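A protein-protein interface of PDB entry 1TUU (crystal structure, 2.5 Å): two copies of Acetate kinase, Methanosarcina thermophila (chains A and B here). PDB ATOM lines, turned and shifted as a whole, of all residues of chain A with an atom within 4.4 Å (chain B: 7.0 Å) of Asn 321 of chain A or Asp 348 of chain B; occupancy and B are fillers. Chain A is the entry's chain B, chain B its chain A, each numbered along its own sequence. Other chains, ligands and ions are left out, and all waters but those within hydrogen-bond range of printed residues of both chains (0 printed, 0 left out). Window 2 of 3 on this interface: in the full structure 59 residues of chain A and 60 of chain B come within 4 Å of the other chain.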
ATOM      1  N   LYS A 203       6.503 -17.616  15.427  1.00  0.00           N
ATOM      2  CA  LYS A 203       5.255 -18.378  15.332  1.00  0.00           C
ATOM      3  C   LYS A 203       5.020 -18.579  13.831  1.00  0.00           C
ATOM      4  O   LYS A 203       4.741 -17.613  13.104  1.00  0.00           O
ATOM      5  CB  LYS A 203       4.109 -17.587  15.965  1.00  0.00           C
ATOM      6  CG  LYS A 203       4.269 -17.396  17.470  1.00  0.00           C
ATOM      7  CD  LYS A 203       3.178 -16.548  18.087  1.00  0.00           C
ATOM      8  CE  LYS A 203       3.133 -15.193  17.439  1.00  0.00           C
ATOM      9  NZ  LYS A 203       1.944 -14.410  17.887  1.00  0.00           N
ATOM     10  N   SER A 317      -4.180 -19.440  12.935  1.00  0.00           N
ATOM     11  CA  SER A 317      -3.840 -18.066  13.254  1.00  0.00           C
ATOM     12  C   SER A 317      -4.372 -17.795  14.651  1.00  0.00           C
ATOM     13  O   SER A 317      -3.845 -16.963  15.383  1.00  0.00           O
ATOM     14  CB  SER A 317      -4.460 -17.124  12.240  1.00  0.00           C
ATOM     15  OG  SER A 317      -3.768 -17.197  11.007  1.00  0.00           O
ATOM     16  N   ALA A 318      -5.421 -18.525  15.009  1.00  0.00           N
ATOM     17  CA  ALA A 318      -6.043 -18.408  16.310  1.00  0.00           C
ATOM     18  C   ALA A 318      -5.260 -19.274  17.292  1.00  0.00           C
ATOM     19  O   ALA A 318      -5.089 -18.909  18.446  1.00  0.00           O
ATOM     20  CB  ALA A 318      -7.487 -18.878  16.243  1.00  0.00           C
ATOM     21  N   VAL A 319      -4.783 -20.425  16.837  1.00  0.00           N
ATOM     22  CA  VAL A 319      -4.033 -21.297  17.712  1.00  0.00           C
ATOM     23  C   VAL A 319      -2.751 -20.633  18.154  1.00  0.00           C
ATOM     24  O   VAL A 319      -2.383 -20.700  19.318  1.00  0.00           O
ATOM     25  CB  VAL A 319      -3.705 -22.624  17.032  1.00  0.00           C
ATOM     26  CG1 VAL A 319      -2.664 -23.378  17.826  1.00  0.00           C
ATOM     27  CG2 VAL A 319      -4.971 -23.461  16.921  1.00  0.00           C
ATOM     28  N   LEU A 320      -2.059 -20.000  17.216  1.00  0.00           N
ATOM     29  CA  LEU A 320      -0.810 -19.315  17.527  1.00  0.00           C
ATOM     30  C   LEU A 320      -1.040 -17.863  17.946  1.00  0.00           C
ATOM     31  O   LEU A 320      -0.081 -17.120  18.134  1.00  0.00           O
ATOM     32  CB  LEU A 320       0.124 -19.368  16.311  1.00  0.00           C
ATOM     33  CG  LEU A 320       0.611 -20.761  15.883  1.00  0.00           C
ATOM     34  CD1 LEU A 320       1.313 -20.692  14.530  1.00  0.00           C
ATOM     35  CD2 LEU A 320       1.549 -21.309  16.933  1.00  0.00           C
ATOM     36  N   ASN A 321      -2.299 -17.461  18.099  1.00  0.00           N
ATOM     37  CA  ASN A 321      -2.598 -16.079  18.459  1.00  0.00           C
ATOM     38  C   ASN A 321      -1.750 -15.171  17.571  1.00  0.00           C
ATOM     39  O   ASN A 321      -0.911 -14.425  18.058  1.00  0.00           O
ATOM     40  CB  ASN A 321      -2.277 -15.798  19.932  1.00  0.00           C
ATOM     41  CG  ASN A 321      -2.754 -14.416  20.381  1.00  0.00           C
ATOM     42  OD1 ASN A 321      -3.477 -13.727  19.653  1.00  0.00           O
ATOM     43  ND2 ASN A 321      -2.367 -14.016  21.590  1.00  0.00           N
ATOM     44  N   GLY A 322      -1.956 -15.281  16.261  1.00  0.00           N
ATOM     45  CA  GLY A 322      -1.202 -14.479  15.324  1.00  0.00           C
ATOM     46  C   GLY A 322       0.086 -15.114  14.824  1.00  0.00           C
ATOM     47  O   GLY A 322       1.003 -15.394  15.601  1.00  0.00           O
ATOM     48  N   LYS B 310     -12.420 -22.009  19.501  1.00  0.00           N
ATOM     49  CA  LYS B 310     -11.423 -21.002  19.200  1.00  0.00           C
ATOM     50  C   LYS B 310     -10.875 -21.203  17.798  1.00  0.00           C
ATOM     51  O   LYS B 310     -10.773 -20.245  17.014  1.00  0.00           O
ATOM     52  CB  LYS B 310     -10.299 -21.072  20.224  1.00  0.00           C
ATOM     53  CG  LYS B 310      -9.101 -20.195  19.933  1.00  0.00           C
ATOM     54  CD  LYS B 310      -8.265 -20.007  21.180  1.00  0.00           C
ATOM     55  CE  LYS B 310      -6.792 -20.063  20.851  1.00  0.00           C
ATOM     56  NZ  LYS B 310      -5.966 -19.263  21.809  1.00  0.00           N
ATOM     57  N   LEU B 344     -12.035 -17.214  24.293  1.00  0.00           N
ATOM     58  CA  LEU B 344     -11.459 -15.970  23.790  1.00  0.00           C
ATOM     59  C   LEU B 344     -10.052 -15.575  24.236  1.00  0.00           C
ATOM     60  O   LEU B 344      -9.471 -14.639  23.691  1.00  0.00           O
ATOM     61  CB  LEU B 344     -12.431 -14.826  24.090  1.00  0.00           C
ATOM     62  CG  LEU B 344     -13.845 -15.133  23.594  1.00  0.00           C
ATOM     63  CD1 LEU B 344     -14.861 -14.316  24.341  1.00  0.00           C
ATOM     64  CD2 LEU B 344     -13.913 -14.883  22.090  1.00  0.00           C
ATOM     65  N   THR B 345      -9.498 -16.259  25.226  1.00  0.00           N
ATOM     66  CA  THR B 345      -8.154 -15.908  25.668  1.00  0.00           C
ATOM     67  C   THR B 345      -7.116 -16.235  24.596  1.00  0.00           C
ATOM     68  O   THR B 345      -7.214 -17.256  23.929  1.00  0.00           O
ATOM     69  CB  THR B 345      -7.771 -16.659  26.943  1.00  0.00           C
ATOM     70  OG1 THR B 345      -8.731 -16.384  27.969  1.00  0.00           O
ATOM     71  CG2 THR B 345      -6.400 -16.224  27.397  1.00  0.00           C
ATOM     72  N   GLY B 346      -6.136 -15.351  24.431  1.00  0.00           N
ATOM     73  CA  GLY B 346      -5.075 -15.550  23.462  1.00  0.00           C
ATOM     74  C   GLY B 346      -5.445 -15.357  22.005  1.00  0.00           C
ATOM     75  O   GLY B 346      -4.977 -16.091  21.130  1.00  0.00           O
ATOM     76  N   LEU B 347      -6.276 -14.359  21.738  1.00  0.00           N
ATOM     77  CA  LEU B 347      -6.725 -14.080  20.385  1.00  0.00           C
ATOM     78  C   LEU B 347      -6.602 -12.593  20.061  1.00  0.00           C
ATOM     79  O   LEU B 347      -7.271 -12.087  19.159  1.00  0.00           O
ATOM     80  CB  LEU B 347      -8.183 -14.530  20.218  1.00  0.00           C
ATOM     81  CG  LEU B 347      -8.474 -16.031  20.320  1.00  0.00           C
ATOM     82  CD1 LEU B 347      -9.965 -16.262  20.254  1.00  0.00           C
ATOM     83  CD2 LEU B 347      -7.775 -16.770  19.188  1.00  0.00           C
ATOM     84  N   ASP B 348      -5.761 -11.890  20.810  1.00  0.00           N
ATOM     85  CA  ASP B 348      -5.586 -10.465  20.574  1.00  0.00           C
ATOM     86  C   ASP B 348      -4.826 -10.275  19.272  1.00  0.00           C
ATOM     87  O   ASP B 348      -4.882  -9.211  18.656  1.00  0.00           O
ATOM     88  CB  ASP B 348      -4.835  -9.815  21.741  1.00  0.00           C
ATOM     89  CG  ASP B 348      -3.602 -10.593  22.149  1.00  0.00           C
ATOM     90  OD1 ASP B 348      -3.744 -11.776  22.552  1.00  0.00           O
ATOM     91  OD2 ASP B 348      -2.494 -10.016  22.068  1.00  0.00           O
ATOM     92  N   GLY B 349      -4.119 -11.324  18.861  1.00  0.00           N
ATOM     93  CA  GLY B 349      -3.376 -11.283  17.617  1.00  0.00           C
ATOM     94  C   GLY B 349      -4.284 -11.288  16.389  1.00  0.00           C
ATOM     95  O   GLY B 349      -3.817 -10.969  15.306  1.00  0.00           O
ATOM     96  N   ILE B 350      -5.555 -11.672  16.534  1.00  0.00           N
ATOM     97  CA  ILE B 350      -6.494 -11.655  15.408  1.00  0.00           C
ATOM     98  C   ILE B 350      -7.609 -10.634  15.671  1.00  0.00           C
ATOM     99  O   ILE B 350      -8.717 -10.740  15.130  1.00  0.00           O
ATOM    100  CB  ILE B 350      -7.153 -13.052  15.127  1.00  0.00           C
ATOM    101  CG1 ILE B 350      -8.137 -13.387  16.245  1.00  0.00           C
ATOM    102  CG2 ILE B 350      -6.085 -14.141  14.972  1.00  0.00           C
ATOM    103  CD1 ILE B 350      -8.878 -14.686  16.035  1.00  0.00           C
ATOM    104  N   GLY B 351      -7.299  -9.658  16.527  1.00  0.00           N
ATOM    105  CA  GLY B 351      -8.217  -8.569  16.855  1.00  0.00           C
ATOM    106  C   GLY B 351      -9.230  -8.771  17.961  1.00  0.00           C
ATOM    107  O   GLY B 351     -10.013  -7.870  18.286  1.00  0.00           O
ATOM    108  N   ILE B 352      -9.215  -9.955  18.549  1.00  0.00           N
ATOM    109  CA  ILE B 352     -10.155 -10.266  19.607  1.00  0.00           C
ATOM    110  C   ILE B 352      -9.535 -10.021  20.975  1.00  0.00           C
ATOM    111  O   ILE B 352      -8.478 -10.544  21.301  1.00  0.00           O
ATOM    112  CB  ILE B 352     -10.654 -11.712  19.470  1.00  0.00           C
ATOM    113  CG1 ILE B 352     -11.407 -11.876  18.143  1.00  0.00           C
ATOM    114  CG2 ILE B 352     -11.571 -12.060  20.597  1.00  0.00           C
ATOM    115  CD1 ILE B 352     -11.883 -13.298  17.860  1.00  0.00           C
ATOM    116  N   LYS B 353     -10.202  -9.188  21.762  1.00  0.00           N
ATOM    117  CA  LYS B 353      -9.742  -8.847  23.099  1.00  0.00           C
ATOM    118  C   LYS B 353     -11.007  -8.693  23.929  1.00  0.00           C
ATOM    119  O   LYS B 353     -12.013  -8.181  23.438  1.00  0.00           O
ATOM    120  CB  LYS B 353      -8.978  -7.519  23.058  1.00  0.00           C
ATOM    121  CG  LYS B 353      -7.886  -7.387  24.096  1.00  0.00           C
ATOM    122  CD  LYS B 353      -7.204  -6.005  24.060  1.00  0.00           C
ATOM    123  CE  LYS B 353      -6.592  -5.672  22.691  1.00  0.00           C
ATOM    124  NZ  LYS B 353      -5.839  -4.378  22.664  1.00  0.00           N
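The backbone NH (N) of Gly 349 of chain B is in hydrogen-bond range of the side-chain amide oxygen (OD1) of Asn 321 of chain A (2.6 Å). The backbone carbonyl oxygen of Gly 346 of chain B lies close to the side-chain amide oxygen of Asn 321 of chain A (3.2 Å). O of Ala 318 of chain A sits close to NZ of Lys 310 of chain B. The side-chain carboxylate (OD1) of Asp 348 of chain B sits at hydrogen-bond distance from the side-chain amide nitrogen (ND2) of Asn 321 of chain A, at 2.8 Å.
Of the 7 printed residues of chain A, 3 touch a printed residue of chain B. Hydrophobic or aromatic side chains of chain B within 4 Å of the printed part of chain A: Leu 347 and Ile 350. Among the printed residues, 8 pairs touch across the chains. Among the printed residues, no Asp or Glu carboxylate lies within 4 Å of a Lys or Arg side-chain nitrogen of the other chain.
No position is printed for both chains. Of the 8 pairs that touch across the chains among the printed residues, none has its exchanged pair printed and touching as well.
The backbone carbonyl oxygen of Leu 347 of chain B is in hydrogen-bond range of the backbone NH of Ile 352 of chain B (2.9 Å). The side-chain amino group (NZ) of Lys 310 of chain B lies within hydrogen-bond range of the backbone carbonyl oxygen (O) of Thr 345 of chain B, at 3.2 Å. The side-chain amino group of Lys 203 of chain A sits at hydrogen-bond distance from the backbone carbonyl oxygen of Asn 321 of chain A (2.9 Å). The backbone NH (N) of Gly 322 of chain A lies within hydrogen-bond range of the backbone carbonyl oxygen (O) of Ser 317 of chain A (2.7 Å). The backbone carbonyl oxygen (O) of Gly 346 of chain B lies within hydrogen-bond range of the side-chain amino group (NZ) of Lys 310 of chain B, at 3.4 Å.
Among the printed residues, merely in contact across the chains: Ser 317 of chain A with Ile 350 of chain B, Ala 318 of chain A with Gly 346 of chain B, Ala 318 of chain A with Leu 347 of chain B and Asn 321 of chain A with Leu 347 of chain B.
Lys 203 of chain A touches none of the printed residues of chain B. Of the printed residues of chain B, Ala 318 of chain A touches Lys 310, Gly 346 and Leu 347. Val 319 of chain A touches none of the printed residues of chain B. Of chain B, only Gly 346, Leu 347, Asp 348 and Gly 349 come within 4 Å of Asn 321 of chain A. Of the printed residues of chain A, Lys 310 of chain B touches Ala 318 (3.2 Å). Of chain A, only Asn 321 (2.8 Å) comes within 4 Å of Asp 348 of chain B. Of the printed residues of chain A, Gly 349 of chain B touches Asn 321 (2.6 Å). Of the printed residues of chain A, Ile 350 of chain B touches Ser 317 (3.6 Å). The nearest printed residue of chain A that does not touch Ile 350 of chain B is Asn 321 of chain A (4.3 Å).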
